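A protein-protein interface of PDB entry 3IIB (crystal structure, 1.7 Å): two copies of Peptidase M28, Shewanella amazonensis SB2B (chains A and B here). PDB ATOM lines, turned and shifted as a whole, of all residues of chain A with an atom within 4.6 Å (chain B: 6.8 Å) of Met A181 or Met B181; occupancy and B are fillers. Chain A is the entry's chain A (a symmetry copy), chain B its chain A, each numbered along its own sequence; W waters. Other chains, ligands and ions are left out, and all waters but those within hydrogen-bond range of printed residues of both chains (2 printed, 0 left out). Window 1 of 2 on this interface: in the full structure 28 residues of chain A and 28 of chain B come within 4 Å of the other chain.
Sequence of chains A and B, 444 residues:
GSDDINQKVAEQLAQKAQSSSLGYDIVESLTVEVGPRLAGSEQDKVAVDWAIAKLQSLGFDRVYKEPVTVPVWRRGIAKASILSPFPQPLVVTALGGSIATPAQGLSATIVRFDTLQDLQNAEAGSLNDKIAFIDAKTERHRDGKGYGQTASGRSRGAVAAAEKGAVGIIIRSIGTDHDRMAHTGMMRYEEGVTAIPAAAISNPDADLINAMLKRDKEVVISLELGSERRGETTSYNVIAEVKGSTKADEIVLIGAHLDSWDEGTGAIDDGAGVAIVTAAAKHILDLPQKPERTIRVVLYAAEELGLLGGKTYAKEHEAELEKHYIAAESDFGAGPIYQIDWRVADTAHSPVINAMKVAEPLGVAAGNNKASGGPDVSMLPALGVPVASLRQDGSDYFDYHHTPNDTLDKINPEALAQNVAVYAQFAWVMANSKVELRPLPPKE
Met A181 touches two residues of chain B. Of chain A, only Arg A180 (3.9 Å) and Met A181 (3.7 Å) come within 4 Å of Met B181. Printed residues of chain A within 4 Å of Asn B405: Asp A179 and Arg A180. Printed residues of chain B within 4 Å of Asp A179: Asn B405 (3.0 Å). Printed residues of chain A within 4 Å of Asp B179: Asn A405. Printed residues of chain B within 4 Å of Arg A180: Met B181 (3.9 Å), Pro B404 (3.0 Å) and Asn B405 (2.8 Å).
Water W1 bridges OD1 of Asp B179 and OD2 of Asp A179. Water W2 lies within hydrogen-bond range of the side-chain carboxylate of Asp A179 (2.8 Å) and the side-chain carboxylate of Asp B179 (2.9 Å).
N of Arg A180 sits at hydrogen-bond distance from OD1 of Asn B405, at 2.8 Å. The side-chain amide nitrogen (ND2) of Asn B405 lies within hydrogen-bond range of the side-chain carboxylate (OD1) of Asp A179, 3.0 Å away. The backbone carbonyl oxygen (O) of Pro B404 lies within hydrogen-bond range of the guanidinium group (NH1) of Arg A180, 3.0 Å away. The backbone carbonyl oxygen (O) of Pro A404 lies within hydrogen-bond range of the guanidinium group (NH1) of Arg B180, 3.0 Å away. The backbone NH (N) of Arg B180 is in hydrogen-bond range of the side-chain amide oxygen (OD1) of Asn A405, 2.8 Å away. The side-chain carboxylate (OD1) of Asp B179 lies within hydrogen-bond range of the side-chain amide nitrogen (ND2) of Asn A405 (3.0 Å).
Arg A180 touches Met B181, and with the chains exchanged Met A181 touches Arg B180. Arg A180 touches Pro B404, and with the chains exchanged Pro A404 touches Arg B180. Arg A180 touches Asn B405, and with the chains exchanged Asn A405 touches Arg B180. Met B181 touches its own counterpart, Met A181. Of the 10 pairs that touch across the chains among the printed residues, 9 have their exchanged pair printed and touching as well.
Arg A180 touches Met B181 (O to CE, 3.9 Å). O of Arg B180 touches CE of Met A181, 3.9 Å away. Met B181 touches Met A181. His B178 touches Asn A405.
Printed residues of chain A that touch a printed residue of chain B: Asp A179, Arg A180, Met A181, Pro A404 and Asn A405. Among the printed residues, no Asp or Glu carboxylate lies within 4 Å of a Lys or Arg side-chain nitrogen of the other chain.
The guanidinium group (NE) of Arg B180 is in salt-bridge range of the side-chain carboxylate (OD2) of Asp B205 (2.9 Å). The side-chain carboxylate (OD2) of Asp A177 sits at hydrogen-bond distance from the backbone NH (N) of Asp A179 (2.9 Å). OG1 of Thr B403 sits at hydrogen-bond distance from N of Asn B405 (2.9 Å). The side-chain carboxylate of Asp B177 sits at hydrogen-bond distance from the backbone NH of Asp B179 (2.9 Å). The side-chain hydroxyl (OG1) of Thr A403 sits at hydrogen-bond distance from the backbone NH (N) of Asn A405, at 2.9 Å.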
ATOM      1  N   SER A 173      16.515 -19.818 -10.455  1.00  0.00           N
ATOM      2  CA  SER A 173      16.557 -19.620  -9.011  1.00  0.00           C
ATOM      3  C   SER A 173      17.744 -20.324  -8.406  1.00  0.00           C
ATOM      4  O   SER A 173      18.065 -21.477  -8.780  1.00  0.00           O
ATOM      5  CB  SER A 173      15.284 -20.139  -8.363  1.00  0.00           C
ATOM      6  OG  SER A 173      14.207 -19.213  -8.533  1.00  0.00           O
ATOM      7  N   ASP A 177      15.789 -27.042  -5.003  1.00  0.00           N
ATOM      8  CA  ASP A 177      14.501 -27.710  -5.222  1.00  0.00           C
ATOM      9  C   ASP A 177      14.134 -27.869  -6.699  1.00  0.00           C
ATOM     10  O   ASP A 177      14.697 -27.211  -7.565  1.00  0.00           O
ATOM     11  CB  ASP A 177      13.428 -26.843  -4.611  1.00  0.00           C
ATOM     12  CG  ASP A 177      13.381 -25.489  -5.251  1.00  0.00           C
ATOM     13  OD1 ASP A 177      14.317 -24.702  -4.960  1.00  0.00           O
ATOM     14  OD2 ASP A 177      12.443 -25.255  -6.065  1.00  0.00           O
ATOM     15  N   ASP A 179      10.748 -27.377  -7.083  1.00  0.00           N
ATOM     16  CA  ASP A 179       9.412 -26.828  -6.856  1.00  0.00           C
ATOM     17  C   ASP A 179       9.183 -25.565  -7.673  1.00  0.00           C
ATOM     18  O   ASP A 179      10.124 -24.882  -8.094  1.00  0.00           O
ATOM     19  CB  ASP A 179       9.235 -26.514  -5.395  1.00  0.00           C
ATOM     20  CG  ASP A 179       9.229 -27.730  -4.527  1.00  0.00           C
ATOM     21  OD1 ASP A 179       8.583 -28.749  -4.910  1.00  0.00           O
ATOM     22  OD2 ASP A 179       9.899 -27.683  -3.462  1.00  0.00           O
ATOM     23  N   ARG A 180       7.904 -25.271  -7.890  1.00  0.00           N
ATOM     24  CA  ARG A 180       7.470 -24.108  -8.646  1.00  0.00           C
ATOM     25  C   ARG A 180       7.514 -22.893  -7.716  1.00  0.00           C
ATOM     26  O   ARG A 180       6.496 -22.233  -7.458  1.00  0.00           O
ATOM     27  CB  ARG A 180       6.101 -24.346  -9.247  1.00  0.00           C
ATOM     28  CG  ARG A 180       5.796 -23.396 -10.373  1.00  0.00           C
ATOM     29  CD  ARG A 180       6.289 -23.966 -11.681  1.00  0.00           C
ATOM     30  NE  ARG A 180       6.081 -23.038 -12.787  1.00  0.00           N
ATOM     31  CZ  ARG A 180       4.929 -22.862 -13.422  1.00  0.00           C
ATOM     32  NH1 ARG A 180       3.846 -23.544 -13.086  1.00  0.00           N
ATOM     33  NH2 ARG A 180       4.877 -21.994 -14.430  1.00  0.00           N
ATOM     34  N   MET A 181       8.733 -22.588  -7.255  1.00  0.00           N
ATOM     35  CA  MET A 181       8.987 -21.532  -6.296  1.00  0.00           C
ATOM     36  C   MET A 181      10.144 -20.706  -6.892  1.00  0.00           C
ATOM     37  O   MET A 181      11.195 -21.265  -7.254  1.00  0.00           O
ATOM     38  CB  MET A 181       9.448 -22.128  -4.955  1.00  0.00           C
ATOM     39  CG  MET A 181       8.416 -23.006  -4.285  1.00  0.00           C
ATOM     40  SD  MET A 181       7.128 -21.995  -3.312  1.00  0.00           S
ATOM     41  CE  MET A 181       6.084 -21.007  -4.529  1.00  0.00           C
ATOM     42  N   ALA A 182       9.941 -19.382  -6.944  1.00  0.00           N
ATOM     43  CA  ALA A 182      10.974 -18.461  -7.371  1.00  0.00           C
ATOM     44  C   ALA A 182      11.708 -17.923  -6.127  1.00  0.00           C
ATOM     45  O   ALA A 182      11.073 -17.509  -5.128  1.00  0.00           O
ATOM     46  CB  ALA A 182      10.406 -17.354  -8.266  1.00  0.00           C
ATOM     47  N   HIS A 183      13.042 -17.995  -6.180  1.00  0.00           N
ATOM     48  CA  HIS A 183      13.887 -17.601  -5.057  1.00  0.00           C
ATOM     49  C   HIS A 183      14.362 -16.161  -5.294  1.00  0.00           C
ATOM     50  O   HIS A 183      14.950 -15.851  -6.341  1.00  0.00           O
ATOM     51  CB  HIS A 183      15.124 -18.479  -4.930  1.00  0.00           C
ATOM     52  CG  HIS A 183      14.879 -19.920  -4.641  1.00  0.00           C
ATOM     53  ND1 HIS A 183      15.461 -20.567  -3.563  1.00  0.00           N
ATOM     54  CD2 HIS A 183      14.171 -20.862  -5.311  1.00  0.00           C
ATOM     55  CE1 HIS A 183      15.140 -21.842  -3.599  1.00  0.00           C
ATOM     56  NE2 HIS A 183      14.350 -22.048  -4.646  1.00  0.00           N
ATOM     57  N   SER A 202      11.401 -20.101 -11.390  1.00  0.00           N
ATOM     58  CA  SER A 202      11.476 -21.368 -10.681  1.00  0.00           C
ATOM     59  C   SER A 202      12.355 -22.307 -11.456  1.00  0.00           C
ATOM     60  O   SER A 202      12.518 -22.180 -12.664  1.00  0.00           O
ATOM     61  CB  SER A 202      10.101 -22.020 -10.456  1.00  0.00           C
ATOM     62  OG  SER A 202       9.545 -22.568 -11.641  1.00  0.00           O
ATOM     63  N   ASN A 203      12.905 -23.278 -10.743  1.00  0.00           N
ATOM     64  CA  ASN A 203      13.670 -24.339 -11.377  1.00  0.00           C
ATOM     65  C   ASN A 203      12.926 -25.097 -12.497  1.00  0.00           C
ATOM     66  O   ASN A 203      13.486 -25.236 -13.576  1.00  0.00           O
ATOM     67  CB  ASN A 203      14.252 -25.240 -10.289  1.00  0.00           C
ATOM     68  CG  ASN A 203      15.612 -24.747  -9.827  1.00  0.00           C
ATOM     69  OD1 ASN A 203      16.610 -24.906 -10.532  1.00  0.00           O
ATOM     70  ND2 ASN A 203      15.636 -24.028  -8.709  1.00  0.00           N
ATOM     71  N   THR A 403      12.354 -18.418  -0.644  1.00  0.00           N
ATOM     72  CA  THR A 403      11.092 -18.688  -1.341  1.00  0.00           C
ATOM     73  C   THR A 403       9.876 -18.391  -0.500  1.00  0.00           C
ATOM     74  O   THR A 403       9.979 -18.268   0.744  1.00  0.00           O
ATOM     75  CB  THR A 403      10.984 -20.180  -1.755  1.00  0.00           C
ATOM     76  OG1 THR A 403      10.742 -20.976  -0.575  1.00  0.00           O
ATOM     77  CG2 THR A 403      12.267 -20.632  -2.512  1.00  0.00           C
ATOM     78  N   PRO A 404       8.687 -18.368  -1.134  1.00  0.00           N
ATOM     79  CA  PRO A 404       7.450 -18.380  -0.333  1.00  0.00           C
ATOM     80  C   PRO A 404       7.236 -19.627   0.514  1.00  0.00           C
ATOM     81  O   PRO A 404       6.321 -19.642   1.327  1.00  0.00           O
ATOM     82  CB  PRO A 404       6.332 -18.254  -1.379  1.00  0.00           C
ATOM     83  CG  PRO A 404       7.038 -17.657  -2.624  1.00  0.00           C
ATOM     84  CD  PRO A 404       8.418 -18.199  -2.583  1.00  0.00           C
ATOM     85  N   ASN A 405       8.037 -20.663   0.268  1.00  0.00           N
ATOM     86  CA  ASN A 405       7.968 -21.900   0.987  1.00  0.00           C
ATOM     87  C   ASN A 405       8.815 -21.901   2.257  1.00  0.00           C
ATOM     88  O   ASN A 405       8.839 -22.905   2.960  1.00  0.00           O
ATOM     89  CB  ASN A 405       8.406 -23.032   0.064  1.00  0.00           C
ATOM     90  CG  ASN A 405       7.592 -24.287   0.219  1.00  0.00           C
ATOM     91  OD1 ASN A 405       6.535 -24.310   0.863  1.00  0.00           O
ATOM     92  ND2 ASN A 405       8.084 -25.377  -0.407  1.00  0.00           N
ATOM     93  N   VAL B  91      -1.111 -17.217   0.116  1.00  0.00           N
ATOM     94  CA  VAL B  91      -0.934 -17.735  -1.241  1.00  0.00           C
ATOM     95  C   VAL B  91      -2.267 -18.460  -1.500  1.00  0.00           C
ATOM     96  O   VAL B  91      -2.662 -19.373  -0.770  1.00  0.00           O
ATOM     97  CB  VAL B  91       0.272 -18.683  -1.408  1.00  0.00           C
ATOM     98  CG1 VAL B  91       0.146 -19.516  -2.695  1.00  0.00           C
ATOM     99  CG2 VAL B  91       1.636 -17.852  -1.418  1.00  0.00           C
ATOM    100  N   VAL B  92      -2.968 -17.964  -2.487  1.00  0.00           N
ATOM    101  CA  VAL B  92      -4.359 -18.324  -2.723  1.00  0.00           C
ATOM    102  C   VAL B  92      -4.523 -18.604  -4.204  1.00  0.00           C
ATOM    103  O   VAL B  92      -3.807 -18.045  -5.032  1.00  0.00           O
ATOM    104  CB  VAL B  92      -5.307 -17.177  -2.258  1.00  0.00           C
ATOM    105  CG1 VAL B  92      -5.136 -15.917  -3.101  1.00  0.00           C
ATOM    106  CG2 VAL B  92      -6.750 -17.591  -2.272  1.00  0.00           C
ATOM    107  N   THR B  93      -5.530 -19.398  -4.534  1.00  0.00           N
ATOM    108  CA  THR B  93      -6.002 -19.488  -5.905  1.00  0.00           C
ATOM    109  C   THR B  93      -7.528 -19.650  -5.934  1.00  0.00           C
ATOM    110  O   THR B  93      -8.117 -20.266  -5.051  1.00  0.00           O
ATOM    111  CB  THR B  93      -5.304 -20.653  -6.651  1.00  0.00           C
ATOM    112  OG1 THR B  93      -5.492 -20.486  -8.064  1.00  0.00           O
ATOM    113  CG2 THR B  93      -5.852 -21.988  -6.184  1.00  0.00           C
ATOM    114  N   SER B 173      -6.398 -25.995   1.012  1.00  0.00           N
ATOM    115  CA  SER B 173      -6.187 -26.744  -0.221  1.00  0.00           C
ATOM    116  C   SER B 173      -6.367 -28.222   0.009  1.00  0.00           C
ATOM    117  O   SER B 173      -5.903 -28.773   1.035  1.00  0.00           O
ATOM    118  CB  SER B 173      -4.792 -26.489  -0.767  1.00  0.00           C
ATOM    119  OG  SER B 173      -4.724 -25.226  -1.436  1.00  0.00           O
ATOM    120  N   ASP B 177       0.418 -31.979   0.616  1.00  0.00           N
ATOM    121  CA  ASP B 177       1.700 -31.297   0.829  1.00  0.00           C
ATOM    122  C   ASP B 177       1.676 -30.291   1.982  1.00  0.00           C
ATOM    123  O   ASP B 177       0.618 -29.875   2.437  1.00  0.00           O
ATOM    124  CB  ASP B 177       2.007 -30.504  -0.417  1.00  0.00           C
ATOM    125  CG  ASP B 177       0.955 -29.473  -0.690  1.00  0.00           C
ATOM    126  OD1 ASP B 177      -0.147 -29.902  -1.118  1.00  0.00           O
ATOM    127  OD2 ASP B 177       1.229 -28.268  -0.428  1.00  0.00           O
ATOM    128  N   HIS B 178       2.863 -29.852   2.422  1.00  0.00           N
ATOM    129  CA  HIS B 178       2.969 -28.620   3.215  1.00  0.00           C
ATOM    130  C   HIS B 178       3.821 -27.615   2.434  1.00  0.00           C
ATOM    131  O   HIS B 178       4.694 -26.935   2.977  1.00  0.00           O
ATOM    132  CB  HIS B 178       3.495 -28.879   4.643  1.00  0.00           C
ATOM    133  CG  HIS B 178       4.819 -29.560   4.707  1.00  0.00           C
ATOM    134  ND1 HIS B 178       5.966 -28.933   5.154  1.00  0.00           N
ATOM    135  CD2 HIS B 178       5.175 -30.842   4.449  1.00  0.00           C
ATOM    136  CE1 HIS B 178       6.977 -29.778   5.111  1.00  0.00           C
ATOM    137  NE2 HIS B 178       6.524 -30.949   4.697  1.00  0.00           N
ATOM    138  N   ASP B 179       3.569 -27.545   1.127  1.00  0.00           N
ATOM    139  CA  ASP B 179       4.174 -26.508   0.292  1.00  0.00           C
ATOM    140  C   ASP B 179       3.262 -25.297   0.163  1.00  0.00           C
ATOM    141  O   ASP B 179       2.042 -25.376   0.353  1.00  0.00           O
ATOM    142  CB  ASP B 179       4.461 -27.062  -1.076  1.00  0.00           C
ATOM    143  CG  ASP B 179       5.516 -28.121  -1.074  1.00  0.00           C
ATOM    144  OD1 ASP B 179       6.553 -27.947  -0.368  1.00  0.00           O
ATOM    145  OD2 ASP B 179       5.300 -29.153  -1.762  1.00  0.00           O
ATOM    146  N   ARG B 180       3.884 -24.167  -0.165  1.00  0.00           N
ATOM    147  CA  ARG B 180       3.197 -22.899  -0.340  1.00  0.00           C
ATOM    148  C   ARG B 180       2.584 -22.880  -1.742  1.00  0.00           C
ATOM    149  O   ARG B 180       2.903 -22.023  -2.581  1.00  0.00           O
ATOM    150  CB  ARG B 180       4.144 -21.744  -0.090  1.00  0.00           C
ATOM    151  CG  ARG B 180       3.416 -20.455   0.179  1.00  0.00           C
ATOM    152  CD  ARG B 180       3.125 -20.322   1.654  1.00  0.00           C
ATOM    153  NE  ARG B 180       2.350 -19.120   1.945  1.00  0.00           N
ATOM    154  CZ  ARG B 180       2.857 -17.897   2.045  1.00  0.00           C
ATOM    155  NH1 ARG B 180       4.152 -17.673   1.884  1.00  0.00           N
ATOM    156  NH2 ARG B 180       2.042 -16.885   2.334  1.00  0.00           N
ATOM    157  N   MET B 181       1.659 -23.823  -1.959  1.00  0.00           N
ATOM    158  CA  MET B 181       1.018 -24.037  -3.240  1.00  0.00           C
ATOM    159  C   MET B 181      -0.493 -24.097  -2.938  1.00  0.00           C
ATOM    160  O   MET B 181      -0.929 -24.870  -2.065  1.00  0.00           O
ATOM    161  CB  MET B 181       1.454 -25.387  -3.837  1.00  0.00           C
ATOM    162  CG  MET B 181       2.932 -25.478  -4.136  1.00  0.00           C
ATOM    163  SD  MET B 181       3.384 -24.674  -5.803  1.00  0.00           S
ATOM    164  CE  MET B 181       3.114 -22.815  -5.676  1.00  0.00           C
ATOM    165  N   ALA B 182      -1.265 -23.306  -3.695  1.00  0.00           N
ATOM    166  CA  ALA B 182      -2.711 -23.332  -3.611  1.00  0.00           C
ATOM    167  C   ALA B 182      -3.258 -24.277  -4.698  1.00  0.00           C
ATOM    168  O   ALA B 182      -2.843 -24.214  -5.880  1.00  0.00           O
ATOM    169  CB  ALA B 182      -3.304 -21.921  -3.679  1.00  0.00           C
ATOM    170  N   HIS B 183      -4.139 -25.186  -4.270  1.00  0.00           N
ATOM    171  CA  HIS B 183      -4.695 -26.206  -5.153  1.00  0.00           C
ATOM    172  C   HIS B 183      -6.060 -25.716  -5.655  1.00  0.00           C
ATOM    173  O   HIS B 183      -6.947 -25.380  -4.855  1.00  0.00           O
ATOM    174  CB  HIS B 183      -4.916 -27.531  -4.437  1.00  0.00           C
ATOM    175  CG  HIS B 183      -3.695 -28.207  -3.916  1.00  0.00           C
ATOM    176  ND1 HIS B 183      -3.376 -29.514  -4.246  1.00  0.00           N
ATOM    177  CD2 HIS B 183      -2.743 -27.794  -3.044  1.00  0.00           C
ATOM    178  CE1 HIS B 183      -2.299 -29.878  -3.584  1.00  0.00           C
ATOM    179  NE2 HIS B 183      -1.889 -28.849  -2.851  1.00  0.00           N
ATOM    180  N   ALA B 200      -8.961 -21.390  -2.624  1.00  0.00           N
ATOM    181  CA  ALA B 200      -8.154 -22.288  -1.788  1.00  0.00           C
ATOM    182  C   ALA B 200      -6.864 -21.575  -1.397  1.00  0.00           C
ATOM    183  O   ALA B 200      -6.272 -20.848  -2.207  1.00  0.00           O
ATOM    184  CB  ALA B 200      -7.832 -23.574  -2.540  1.00  0.00           C
ATOM    185  N   ILE B 201      -6.436 -21.792  -0.148  1.00  0.00           N
ATOM    186  CA  ILE B 201      -5.176 -21.267   0.336  1.00  0.00           C
ATOM    187  C   ILE B 201      -4.237 -22.429   0.576  1.00  0.00           C
ATOM    188  O   ILE B 201      -4.678 -23.588   0.666  1.00  0.00           O
ATOM    189  CB  ILE B 201      -5.315 -20.379   1.583  1.00  0.00           C
ATOM    190  CG1 ILE B 201      -5.770 -21.195   2.823  1.00  0.00           C
ATOM    191  CG2 ILE B 201      -6.229 -19.198   1.294  1.00  0.00           C
ATOM    192  CD1 ILE B 201      -6.045 -20.351   4.093  1.00  0.00           C
ATOM    193  N   SER B 202      -2.936 -22.132   0.576  1.00  0.00           N
ATOM    194  CA  SER B 202      -1.943 -23.179   0.754  1.00  0.00           C
ATOM    195  C   SER B 202      -2.111 -23.782   2.119  1.00  0.00           C
ATOM    196  O   SER B 202      -2.623 -23.153   3.037  1.00  0.00           O
ATOM    197  CB  SER B 202      -0.498 -22.680   0.587  1.00  0.00           C
ATOM    198  OG  SER B 202      -0.051 -21.894   1.681  1.00  0.00           O
ATOM    199  N   ASN B 203      -1.645 -25.014   2.249  1.00  0.00           N
ATOM    200  CA  ASN B 203      -1.615 -25.677   3.543  1.00  0.00           C
ATOM    201  C   ASN B 203      -0.880 -24.899   4.655  1.00  0.00           C
ATOM    202  O   ASN B 203      -1.451 -24.737   5.725  1.00  0.00           O
ATOM    203  CB  ASN B 203      -1.121 -27.110   3.348  1.00  0.00           C
ATOM    204  CG  ASN B 203      -2.271 -28.060   3.061  1.00  0.00           C
ATOM    205  OD1 ASN B 203      -3.031 -28.416   3.963  1.00  0.00           O
ATOM    206  ND2 ASN B 203      -2.484 -28.368   1.785  1.00  0.00           N
ATOM    207  N   PRO B 204       0.329 -24.327   4.383  1.00  0.00           N
ATOM    208  CA  PRO B 204       0.983 -23.504   5.421  1.00  0.00           C
ATOM    209  C   PRO B 204       0.138 -22.278   5.804  1.00  0.00           C
ATOM    210  O   PRO B 204       0.100 -21.878   6.952  1.00  0.00           O
ATOM    211  CB  PRO B 204       2.312 -23.119   4.765  1.00  0.00           C
ATOM    212  CG  PRO B 204       2.599 -24.313   3.838  1.00  0.00           C
ATOM    213  CD  PRO B 204       1.244 -24.604   3.258  1.00  0.00           C
ATOM    214  N   ASP B 205      -0.568 -21.694   4.833  1.00  0.00           N
ATOM    215  CA  ASP B 205      -1.409 -20.545   5.147  1.00  0.00           C
ATOM    216  C   ASP B 205      -2.611 -20.915   6.057  1.00  0.00           C
ATOM    217  O   ASP B 205      -3.014 -20.162   6.932  1.00  0.00           O
ATOM    218  CB  ASP B 205      -1.892 -19.889   3.842  1.00  0.00           C
ATOM    219  CG  ASP B 205      -0.801 -19.139   3.147  1.00  0.00           C
ATOM    220  OD1 ASP B 205      -0.199 -18.248   3.793  1.00  0.00           O
ATOM    221  OD2 ASP B 205      -0.559 -19.444   1.953  1.00  0.00           O
ATOM    222  N   ASP B 399       0.269 -34.188  -3.406  1.00  0.00           N
ATOM    223  CA  ASP B 399       1.258 -33.120  -3.182  1.00  0.00           C
ATOM    224  C   ASP B 399       1.306 -32.128  -4.344  1.00  0.00           C
ATOM    225  O   ASP B 399       1.652 -30.969  -4.130  1.00  0.00           O
ATOM    226  CB  ASP B 399       2.644 -33.650  -2.953  1.00  0.00           C
ATOM    227  CG  ASP B 399       2.757 -34.519  -1.707  1.00  0.00           C
ATOM    228  OD1 ASP B 399       1.849 -34.511  -0.852  1.00  0.00           O
ATOM    229  OD2 ASP B 399       3.782 -35.207  -1.590  1.00  0.00           O
ATOM    230  N   THR B 403      -1.942 -28.037  -8.553  1.00  0.00           N
ATOM    231  CA  THR B 403      -1.072 -26.916  -8.182  1.00  0.00           C
ATOM    232  C   THR B 403      -0.220 -26.424  -9.325  1.00  0.00           C
ATOM    233  O   THR B 403      -0.050 -27.136 -10.343  1.00  0.00           O
ATOM    234  CB  THR B 403      -0.093 -27.313  -7.045  1.00  0.00           C
ATOM    235  OG1 THR B 403       0.920 -28.188  -7.585  1.00  0.00           O
ATOM    236  CG2 THR B 403      -0.864 -27.969  -5.864  1.00  0.00           C
ATOM    237  N   PRO B 404       0.417 -25.249  -9.149  1.00  0.00           N
ATOM    238  CA  PRO B 404       1.484 -24.866 -10.092  1.00  0.00           C
ATOM    239  C   PRO B 404       2.696 -25.787 -10.110  1.00  0.00           C
ATOM    240  O   PRO B 404       3.547 -25.630 -10.976  1.00  0.00           O
ATOM    241  CB  PRO B 404       1.894 -23.459  -9.633  1.00  0.00           C
ATOM    242  CG  PRO B 404       0.681 -22.956  -8.809  1.00  0.00           C
ATOM    243  CD  PRO B 404       0.111 -24.171  -8.178  1.00  0.00           C
ATOM    244  N   ASN B 405       2.785 -26.680  -9.125  1.00  0.00           N
ATOM    245  CA  ASN B 405       3.859 -27.621  -9.011  1.00  0.00           C
ATOM    246  C   ASN B 405       3.607 -28.911  -9.786  1.00  0.00           C
ATOM    247  O   ASN B 405       4.454 -29.798  -9.766  1.00  0.00           O
ATOM    248  CB  ASN B 405       4.086 -27.933  -7.535  1.00  0.00           C
ATOM    249  CG  ASN B 405       5.537 -28.059  -7.161  1.00  0.00           C
ATOM    250  OD1 ASN B 405       6.446 -27.715  -7.928  1.00  0.00           O
ATOM    251  ND2 ASN B 405       5.776 -28.554  -5.929  1.00  0.00           N
ATOM    252  N   ASP B 406       2.487 -29.025 -10.507  1.00  0.00           N
ATOM    253  CA  ASP B 406       2.243 -30.193 -11.382  1.00  0.00           C
ATOM    254  C   ASP B 406       3.019 -30.046 -12.689  1.00  0.00           C
ATOM    255  O   ASP B 406       2.484 -29.582 -13.724  1.00  0.00           O
ATOM    256  CB  ASP B 406       0.756 -30.416 -11.635  1.00  0.00           C
ATOM    257  CG  ASP B 406       0.515 -31.653 -12.466  1.00  0.00           C
ATOM    258  OD1 ASP B 406       1.531 -32.344 -12.706  1.00  0.00           O
ATOM    259  OD2 ASP B 406      -0.641 -31.951 -12.844  1.00  0.00           O
HETATM  260  O   HOH W   1       9.035 -28.961  -1.033  1.00  0.00           O
HETATM  261  O   HOH W   2       7.392 -30.537  -3.172  1.00  0.00           O
